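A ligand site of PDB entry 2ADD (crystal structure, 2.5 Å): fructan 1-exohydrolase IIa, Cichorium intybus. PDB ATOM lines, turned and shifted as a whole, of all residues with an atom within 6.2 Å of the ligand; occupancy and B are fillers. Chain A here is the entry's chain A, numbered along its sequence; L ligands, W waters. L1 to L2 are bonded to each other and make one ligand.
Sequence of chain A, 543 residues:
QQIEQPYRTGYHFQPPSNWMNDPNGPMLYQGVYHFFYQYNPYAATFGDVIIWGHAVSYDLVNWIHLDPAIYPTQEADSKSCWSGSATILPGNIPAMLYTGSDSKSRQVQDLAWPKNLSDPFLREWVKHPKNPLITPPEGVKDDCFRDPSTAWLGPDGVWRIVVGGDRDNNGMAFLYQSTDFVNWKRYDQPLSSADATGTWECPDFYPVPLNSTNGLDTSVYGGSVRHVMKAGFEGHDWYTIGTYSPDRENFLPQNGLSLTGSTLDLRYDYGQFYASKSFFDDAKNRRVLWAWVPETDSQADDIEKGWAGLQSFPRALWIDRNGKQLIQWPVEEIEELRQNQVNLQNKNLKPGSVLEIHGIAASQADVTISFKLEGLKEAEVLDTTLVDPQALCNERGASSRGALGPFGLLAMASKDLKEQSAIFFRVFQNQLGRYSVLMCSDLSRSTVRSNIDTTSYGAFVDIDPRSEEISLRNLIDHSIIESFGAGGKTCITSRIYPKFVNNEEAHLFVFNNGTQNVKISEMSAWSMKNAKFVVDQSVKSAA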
ATOM      1  N   TRP A  19      17.504  13.541   9.721  1.00  0.00           N
ATOM      2  CA  TRP A  19      16.689  14.728   9.848  1.00  0.00           C
ATOM      3  C   TRP A  19      16.156  15.322   8.558  1.00  0.00           C
ATOM      4  O   TRP A  19      16.866  15.424   7.547  1.00  0.00           O
ATOM      5  CB  TRP A  19      17.473  15.797  10.607  1.00  0.00           C
ATOM      6  CG  TRP A  19      16.874  17.178  10.561  1.00  0.00           C
ATOM      7  CD1 TRP A  19      16.841  18.027   9.485  1.00  0.00           C
ATOM      8  CD2 TRP A  19      16.235  17.866  11.639  1.00  0.00           C
ATOM      9  NE1 TRP A  19      16.229  19.206   9.837  1.00  0.00           N
ATOM     10  CE2 TRP A  19      15.845  19.133  11.154  1.00  0.00           C
ATOM     11  CE3 TRP A  19      15.953  17.534  12.972  1.00  0.00           C
ATOM     12  CZ2 TRP A  19      15.191  20.081  11.955  1.00  0.00           C
ATOM     13  CZ3 TRP A  19      15.299  18.482  13.773  1.00  0.00           C
ATOM     14  CH2 TRP A  19      14.926  19.732  13.253  1.00  0.00           C
ATOM     15  N   ASN A  21      13.340  18.637   7.415  1.00  0.00           N
ATOM     16  CA  ASN A  21      12.402  19.675   7.813  1.00  0.00           C
ATOM     17  C   ASN A  21      11.605  20.195   6.615  1.00  0.00           C
ATOM     18  O   ASN A  21      10.863  19.428   5.990  1.00  0.00           O
ATOM     19  CB  ASN A  21      13.057  20.806   8.659  1.00  0.00           C
ATOM     20  CG  ASN A  21      14.278  21.458   8.007  1.00  0.00           C
ATOM     21  OD1 ASN A  21      15.293  20.817   7.749  1.00  0.00           O
ATOM     22  ND2 ASN A  21      14.186  22.763   7.758  1.00  0.00           N
ATOM     23  N   ASP A  22      11.773  21.456   6.250  1.00  0.00           N
ATOM     24  CA  ASP A  22      11.002  22.091   5.169  1.00  0.00           C
ATOM     25  C   ASP A  22      10.847  21.431   3.787  1.00  0.00           C
ATOM     26  O   ASP A  22      11.812  21.005   3.160  1.00  0.00           O
ATOM     27  CB  ASP A  22      11.530  23.508   4.948  1.00  0.00           C
ATOM     28  CG  ASP A  22      11.493  24.346   6.204  1.00  0.00           C
ATOM     29  OD1 ASP A  22      11.406  23.773   7.316  1.00  0.00           O
ATOM     30  OD2 ASP A  22      11.568  25.590   6.076  1.00  0.00           O
ATOM     31  N   ASN A  24      10.547  21.321  -0.099  1.00  0.00           N
ATOM     32  CA  ASN A  24      11.111  22.225  -1.095  1.00  0.00           C
ATOM     33  C   ASN A  24      10.716  21.884  -2.534  1.00  0.00           C
ATOM     34  O   ASN A  24      10.480  20.725  -2.872  1.00  0.00           O
ATOM     35  CB  ASN A  24      12.645  22.216  -1.017  1.00  0.00           C
ATOM     36  CG  ASN A  24      13.174  22.744   0.312  1.00  0.00           C
ATOM     37  OD1 ASN A  24      14.274  22.392   0.724  1.00  0.00           O
ATOM     38  ND2 ASN A  24      12.402  23.612   0.975  1.00  0.00           N
ATOM     39  N   GLN A  38      14.455  19.832   2.995  1.00  0.00           N
ATOM     40  CA  GLN A  38      15.643  20.149   3.750  1.00  0.00           C
ATOM     41  C   GLN A  38      16.067  18.846   4.426  1.00  0.00           C
ATOM     42  O   GLN A  38      15.282  18.223   5.147  1.00  0.00           O
ATOM     43  CB  GLN A  38      15.330  21.233   4.783  1.00  0.00           C
ATOM     44  CG  GLN A  38      15.018  22.571   4.147  1.00  0.00           C
ATOM     45  CD  GLN A  38      16.246  23.196   3.513  1.00  0.00           C
ATOM     46  OE1 GLN A  38      17.049  23.839   4.183  1.00  0.00           O
ATOM     47  NE2 GLN A  38      16.399  22.999   2.207  1.00  0.00           N
ATOM     48  N   PHE A  46      19.214  19.117  13.307  1.00  0.00           N
ATOM     49  CA  PHE A  46      19.587  20.126  12.329  1.00  0.00           C
ATOM     50  C   PHE A  46      21.118  20.161  12.309  1.00  0.00           C
ATOM     51  O   PHE A  46      21.757  19.683  13.259  1.00  0.00           O
ATOM     52  CB  PHE A  46      19.037  21.496  12.722  1.00  0.00           C
ATOM     53  CG  PHE A  46      19.076  22.494  11.600  1.00  0.00           C
ATOM     54  CD1 PHE A  46      18.250  22.343  10.480  1.00  0.00           C
ATOM     55  CD2 PHE A  46      19.950  23.574  11.643  1.00  0.00           C
ATOM     56  CE1 PHE A  46      18.299  23.249   9.427  1.00  0.00           C
ATOM     57  CE2 PHE A  46      20.003  24.496  10.595  1.00  0.00           C
ATOM     58  CZ  PHE A  46      19.168  24.334   9.476  1.00  0.00           C
ATOM     59  N   ILE A  50      22.996  21.347   5.353  1.00  0.00           N
ATOM     60  CA  ILE A  50      21.641  20.957   4.990  1.00  0.00           C
ATOM     61  C   ILE A  50      21.537  20.967   3.466  1.00  0.00           C
ATOM     62  O   ILE A  50      21.961  21.922   2.817  1.00  0.00           O
ATOM     63  CB  ILE A  50      20.589  21.930   5.567  1.00  0.00           C
ATOM     64  CG1 ILE A  50      20.524  21.791   7.091  1.00  0.00           C
ATOM     65  CG2 ILE A  50      19.225  21.663   4.934  1.00  0.00           C
ATOM     66  CD1 ILE A  50      20.088  20.411   7.572  1.00  0.00           C
ATOM     67  N   CYS A  81      22.243  24.550   1.516  1.00  0.00           N
ATOM     68  CA  CYS A  81      21.232  24.854   0.514  1.00  0.00           C
ATOM     69  C   CYS A  81      19.886  24.819   1.232  1.00  0.00           C
ATOM     70  O   CYS A  81      19.297  23.759   1.431  1.00  0.00           O
ATOM     71  CB  CYS A  81      21.256  23.815  -0.604  1.00  0.00           C
ATOM     72  SG  CYS A  81      22.790  23.839  -1.577  1.00  0.00           S
ATOM     73  N   TRP A  82      19.398  25.993   1.624  1.00  0.00           N
ATOM     74  CA  TRP A  82      18.140  26.060   2.325  1.00  0.00           C
ATOM     75  C   TRP A  82      16.920  26.152   1.404  1.00  0.00           C
ATOM     76  O   TRP A  82      17.042  26.049   0.179  1.00  0.00           O
ATOM     77  CB  TRP A  82      18.195  27.200   3.351  1.00  0.00           C
ATOM     78  CG  TRP A  82      19.233  26.909   4.434  1.00  0.00           C
ATOM     79  CD1 TRP A  82      19.495  25.682   5.012  1.00  0.00           C
ATOM     80  CD2 TRP A  82      20.116  27.835   5.071  1.00  0.00           C
ATOM     81  NE1 TRP A  82      20.480  25.802   5.957  1.00  0.00           N
ATOM     82  CE2 TRP A  82      20.878  27.119   6.019  1.00  0.00           C
ATOM     83  CE3 TRP A  82      20.335  29.225   4.937  1.00  0.00           C
ATOM     84  CZ2 TRP A  82      21.854  27.725   6.828  1.00  0.00           C
ATOM     85  CZ3 TRP A  82      21.304  29.830   5.740  1.00  0.00           C
ATOM     86  CH2 TRP A  82      22.049  29.079   6.671  1.00  0.00           C
ATOM     87  N   SER A  83      15.739  26.334   1.995  1.00  0.00           N
ATOM     88  CA  SER A  83      14.473  26.362   1.264  1.00  0.00           C
ATOM     89  C   SER A  83      14.324  27.168  -0.020  1.00  0.00           C
ATOM     90  O   SER A  83      14.926  28.224  -0.202  1.00  0.00           O
ATOM     91  CB  SER A  83      13.343  26.723   2.226  1.00  0.00           C
ATOM     92  OG  SER A  83      13.232  25.728   3.221  1.00  0.00           O
ATOM     93  N   GLY A  84      13.493  26.635  -0.915  1.00  0.00           N
ATOM     94  CA  GLY A  84      13.244  27.271  -2.194  1.00  0.00           C
ATOM     95  C   GLY A  84      11.993  26.704  -2.864  1.00  0.00           C
ATOM     96  O   GLY A  84      11.348  25.804  -2.329  1.00  0.00           O
ATOM     97  N   THR A  99      17.420  29.452  -1.223  1.00  0.00           N
ATOM     98  CA  THR A  99      18.306  30.284  -0.419  1.00  0.00           C
ATOM     99  C   THR A  99      19.563  29.504  -0.095  1.00  0.00           C
ATOM    100  O   THR A  99      19.500  28.400   0.438  1.00  0.00           O
ATOM    101  CB  THR A  99      17.667  30.687   0.912  1.00  0.00           C
ATOM    102  OG1 THR A  99      16.489  31.456   0.657  1.00  0.00           O
ATOM    103  CG2 THR A  99      18.661  31.509   1.727  1.00  0.00           C
ATOM    104  N   GLN A 107      22.602  34.896   3.598  1.00  0.00           N
ATOM    105  CA  GLN A 107      21.498  34.177   2.985  1.00  0.00           C
ATOM    106  C   GLN A 107      21.266  34.897   1.672  1.00  0.00           C
ATOM    107  O   GLN A 107      20.943  36.084   1.642  1.00  0.00           O
ATOM    108  CB  GLN A 107      20.258  34.226   3.876  1.00  0.00           C
ATOM    109  CG  GLN A 107      20.513  33.614   5.259  1.00  0.00           C
ATOM    110  CD  GLN A 107      19.283  33.520   6.133  1.00  0.00           C
ATOM    111  OE1 GLN A 107      18.299  34.221   5.929  1.00  0.00           O
ATOM    112  NE2 GLN A 107      19.355  32.651   7.146  1.00  0.00           N
ATOM    113  N   ASP A 143      21.118  37.284   7.755  1.00  0.00           N
ATOM    114  CA  ASP A 143      20.435  36.046   8.109  1.00  0.00           C
ATOM    115  C   ASP A 143      18.931  36.237   8.292  1.00  0.00           C
ATOM    116  O   ASP A 143      18.281  35.494   9.040  1.00  0.00           O
ATOM    117  CB  ASP A 143      21.057  35.453   9.382  1.00  0.00           C
ATOM    118  CG  ASP A 143      20.914  36.360  10.587  1.00  0.00           C
ATOM    119  OD1 ASP A 143      21.307  35.922  11.687  1.00  0.00           O
ATOM    120  OD2 ASP A 143      20.430  37.501  10.447  1.00  0.00           O
ATOM    121  N   ARG A 146      15.293  35.053   3.224  1.00  0.00           N
ATOM    122  CA  ARG A 146      15.259  33.727   2.630  1.00  0.00           C
ATOM    123  C   ARG A 146      13.907  33.193   2.157  1.00  0.00           C
ATOM    124  O   ARG A 146      12.862  33.834   2.283  1.00  0.00           O
ATOM    125  CB  ARG A 146      15.817  32.733   3.642  1.00  0.00           C
ATOM    126  CG  ARG A 146      15.062  32.778   4.977  1.00  0.00           C
ATOM    127  CD  ARG A 146      15.576  31.737   5.959  1.00  0.00           C
ATOM    128  NE  ARG A 146      14.950  31.873   7.277  1.00  0.00           N
ATOM    129  CZ  ARG A 146      15.162  32.892   8.112  1.00  0.00           C
ATOM    130  NH1 ARG A 146      15.990  33.867   7.768  1.00  0.00           N
ATOM    131  NH2 ARG A 146      14.543  32.929   9.280  1.00  0.00           N
ATOM    132  N   ASP A 147      13.964  31.977   1.610  1.00  0.00           N
ATOM    133  CA  ASP A 147      12.820  31.218   1.118  1.00  0.00           C
ATOM    134  C   ASP A 147      12.022  31.810  -0.033  1.00  0.00           C
ATOM    135  O   ASP A 147      10.854  32.172   0.132  1.00  0.00           O
ATOM    136  CB  ASP A 147      11.877  30.918   2.291  1.00  0.00           C
ATOM    137  CG  ASP A 147      12.616  30.428   3.523  1.00  0.00           C
ATOM    138  OD1 ASP A 147      13.728  29.869   3.398  1.00  0.00           O
ATOM    139  OD2 ASP A 147      12.068  30.585   4.639  1.00  0.00           O
ATOM    140  N   GLU A 201       8.938  33.353   7.253  1.00  0.00           N
ATOM    141  CA  GLU A 201       9.557  32.177   6.664  1.00  0.00           C
ATOM    142  C   GLU A 201       8.691  31.446   5.641  1.00  0.00           C
ATOM    143  O   GLU A 201       7.465  31.320   5.810  1.00  0.00           O
ATOM    144  CB  GLU A 201       9.997  31.232   7.786  1.00  0.00           C
ATOM    145  CG  GLU A 201      11.064  31.847   8.693  1.00  0.00           C
ATOM    146  CD  GLU A 201      11.530  30.916   9.791  1.00  0.00           C
ATOM    147  OE1 GLU A 201      12.715  30.993  10.165  1.00  0.00           O
ATOM    148  OE2 GLU A 201      10.714  30.112  10.286  1.00  0.00           O
ATOM    149  N   CYS A 202       9.324  30.968   4.570  1.00  0.00           N
ATOM    150  CA  CYS A 202       8.645  30.248   3.495  1.00  0.00           C
ATOM    151  C   CYS A 202       7.351  30.894   3.060  1.00  0.00           C
ATOM    152  O   CYS A 202       6.282  30.290   3.141  1.00  0.00           O
ATOM    153  CB  CYS A 202       8.382  28.802   3.934  1.00  0.00           C
ATOM    154  SG  CYS A 202       9.891  27.903   4.350  1.00  0.00           S
ATOM    155  N   TYR A 274       4.353  23.274   9.867  1.00  0.00           N
ATOM    156  CA  TYR A 274       5.172  24.451   9.570  1.00  0.00           C
ATOM    157  C   TYR A 274       5.879  24.415   8.212  1.00  0.00           C
ATOM    158  O   TYR A 274       6.096  23.350   7.618  1.00  0.00           O
ATOM    159  CB  TYR A 274       6.212  24.656  10.689  1.00  0.00           C
ATOM    160  CG  TYR A 274       6.795  26.056  10.710  1.00  0.00           C
ATOM    161  CD1 TYR A 274       6.009  27.141  11.108  1.00  0.00           C
ATOM    162  CD2 TYR A 274       8.108  26.308  10.276  1.00  0.00           C
ATOM    163  CE1 TYR A 274       6.498  28.445  11.066  1.00  0.00           C
ATOM    164  CE2 TYR A 274       8.613  27.616  10.228  1.00  0.00           C
ATOM    165  CZ  TYR A 274       7.801  28.686  10.632  1.00  0.00           C
ATOM    166  OH  TYR A 274       8.267  29.984  10.573  1.00  0.00           O
ATOM    167  N   ALA A 275       6.251  25.597   7.730  1.00  0.00           N
ATOM    168  CA  ALA A 275       6.946  25.726   6.454  1.00  0.00           C
ATOM    169  C   ALA A 275       6.161  25.126   5.292  1.00  0.00           C
ATOM    170  O   ALA A 275       6.729  24.623   4.320  1.00  0.00           O
ATOM    171  CB  ALA A 275       8.330  25.060   6.547  1.00  0.00           C
ATOM    172  N   TRP A 292       5.900  20.504   6.759  1.00  0.00           N
ATOM    173  CA  TRP A 292       6.799  19.779   7.627  1.00  0.00           C
ATOM    174  C   TRP A 292       6.105  19.628   8.978  1.00  0.00           C
ATOM    175  O   TRP A 292       5.493  20.573   9.479  1.00  0.00           O
ATOM    176  CB  TRP A 292       8.115  20.553   7.789  1.00  0.00           C
ATOM    177  CG  TRP A 292       8.988  20.097   8.929  1.00  0.00           C
ATOM    178  CD1 TRP A 292       9.403  18.815   9.195  1.00  0.00           C
ATOM    179  CD2 TRP A 292       9.557  20.921   9.947  1.00  0.00           C
ATOM    180  NE1 TRP A 292      10.195  18.798  10.313  1.00  0.00           N
ATOM    181  CE2 TRP A 292      10.312  20.079  10.791  1.00  0.00           C
ATOM    182  CE3 TRP A 292       9.517  22.302  10.224  1.00  0.00           C
ATOM    183  CZ2 TRP A 292      11.006  20.569  11.906  1.00  0.00           C
ATOM    184  CZ3 TRP A 292      10.210  22.785  11.327  1.00  0.00           C
ATOM    185  CH2 TRP A 292      10.942  21.915  12.160  1.00  0.00           C
HETATM  186  C1  LIG L   1      15.466  27.982   9.923  1.00  0.00           C
HETATM  187  C2  LIG L   1      15.484  28.987  11.099  1.00  0.00           C
HETATM  188  C3  LIG L   1      16.072  30.332  10.647  1.00  0.00           C
HETATM  189  C4  LIG L   1      17.480  30.069  10.136  1.00  0.00           C
HETATM  190  C5  LIG L   1      17.433  29.063   8.966  1.00  0.00           C
HETATM  191  C6  LIG L   1      18.816  28.734   8.408  1.00  0.00           C
HETATM  192  O1  LIG L   1      14.150  29.153  11.593  1.00  0.00           O
HETATM  193  O2  LIG L   1      16.112  31.264  11.748  1.00  0.00           O
HETATM  194  O3  LIG L   1      18.050  31.300   9.712  1.00  0.00           O
HETATM  195  O4  LIG L   1      16.831  27.824   9.383  1.00  0.00           O
HETATM  196  O5  LIG L   1      19.601  28.125   9.426  1.00  0.00           O
HETATM  197  C1  LG2 L   2      12.583  26.804   8.688  1.00  0.00           C
HETATM  198  C2  LG2 L   2      13.844  27.444   8.071  1.00  0.00           C
HETATM  199  C3  LG2 L   2      13.630  28.125   6.677  1.00  0.00           C
HETATM  200  C4  LG2 L   2      14.947  27.824   5.975  1.00  0.00           C
HETATM  201  C5  LG2 L   2      15.151  26.393   6.494  1.00  0.00           C
HETATM  202  C6  LG2 L   2      16.589  25.894   6.542  1.00  0.00           C
HETATM  203  O1  LG2 L   2      11.580  27.746   9.000  1.00  0.00           O
HETATM  204  O2  LG2 L   2      14.520  28.441   8.882  1.00  0.00           O
HETATM  205  O3  LG2 L   2      13.431  29.540   6.780  1.00  0.00           O
HETATM  206  O4  LG2 L   2      14.847  27.849   4.543  1.00  0.00           O
HETATM  207  O5  LG2 L   2      14.690  26.338   7.823  1.00  0.00           O
HETATM  208  O6  LG2 L   2      16.550  24.491   6.796  1.00  0.00           O
HETATM  209  O   HOH W   1      18.661  27.301  12.196  1.00  0.00           O
HETATM  210  O   HOH W   2      12.742  24.147  10.225  1.00  0.00           O
HETATM  211  O   HOH W   3      18.007  33.891  11.489  1.00  0.00           O
HETATM  212  O   HOH W   4      11.146  28.816  12.994  1.00  0.00           O
HETATM  213  O   HOH W   5      21.448  30.292  10.205  1.00  0.00           O
HETATM  214  O   HOH W   6      13.917  30.740  13.868  1.00  0.00           O
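OD1 of Asp 147 is in hydrogen-bond range of O4 of LG2 L2 (2.6 Å). An oxygen (O3) of LG2 L2 lies within hydrogen-bond range of the guanidinium group (NE) of Arg 146, at 2.8 Å. O6 of LG2 L2 sits at hydrogen-bond distance from OE1 of Gln 38, at 2.7 Å. The side-chain amide nitrogen (NE2) of Gln 107 is in hydrogen-bond range of an oxygen (O3) of LIG L1. O4 of LG2 L2 sits close to N of Ser 83 (3.1 Å). OG of Ser 83 sits at hydrogen-bond distance from O4 of LG2 L2, 3.0 Å away. OE1 of Glu 201 lies within hydrogen-bond range of O1 of LIG L1 (2.7 Å). ND2 of Asn 21 sits at hydrogen-bond distance from O6 of LG2 L2 (3.1 Å).
O of Ser 83 sits at hydrogen-bond distance from N of Thr 99, 3.0 Å away. OD1 of Asn 24 sits at hydrogen-bond distance from NE2 of Gln 38 (2.7 Å). ND2 of Asn 21 lies within hydrogen-bond range of OD1 of Asp 22 (3.0 Å). The side-chain sulfur (SG) of Cys 202 sits at hydrogen-bond distance from the side-chain carboxylate (OD2) of Asp 22. The backbone carbonyl oxygen of Asp 22 sits at hydrogen-bond distance from the side-chain amide nitrogen of Asn 24 (3.5 Å). The backbone NH (N) of Trp 82 lies within hydrogen-bond range of the backbone carbonyl oxygen (O) of Thr 99, 2.7 Å away. The side-chain amide oxygen (OD1) of Asn 21 is in hydrogen-bond range of the indole nitrogen (NE1) of Trp 19, at 2.8 Å. The guanidinium group (NH1) of Arg 146 lies within hydrogen-bond range of the side-chain amide oxygen (OE1) of Gln 107 (3.0 Å).
Water W2 bridges the side-chain amide nitrogen (ND2) of Asn 21 (3.2 Å) and the side-chain carboxylate (OD1) of Asp 22 (3.2 Å). Water W3 lies within hydrogen-bond range of the backbone carbonyl oxygen (O) of Asp 143 (2.9 Å) and an oxygen (O3) of LIG L1 (3.1 Å). Water W4 bridges the side-chain carboxylate of Glu 201 (3.0 Å) and an oxygen (O1) of LIG L1 (3.3 Å).
Asp 22 touches the ligand. CE1 of Phe 46 touches O6 of LG2 L2, at 3.4 Å. Trp 82 touches the ligand. CE2 of Tyr 274 touches O1 of LG2 L2, 3.2 Å away. Hydrophobic or aromatic side chains that line the ligand: Phe 46, Trp 82 and Tyr 274. 11 residues have an atom within 4 Å of the ligand: Asn 21, Asp 22, Gln 38, Phe 46, Trp 82, Ser 83, Gln 107, Arg 146, Asp 147, Glu 201 and Tyr 274. The nearest printed residue that does not touch the ligand is Asp 143 (4.3 Å).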
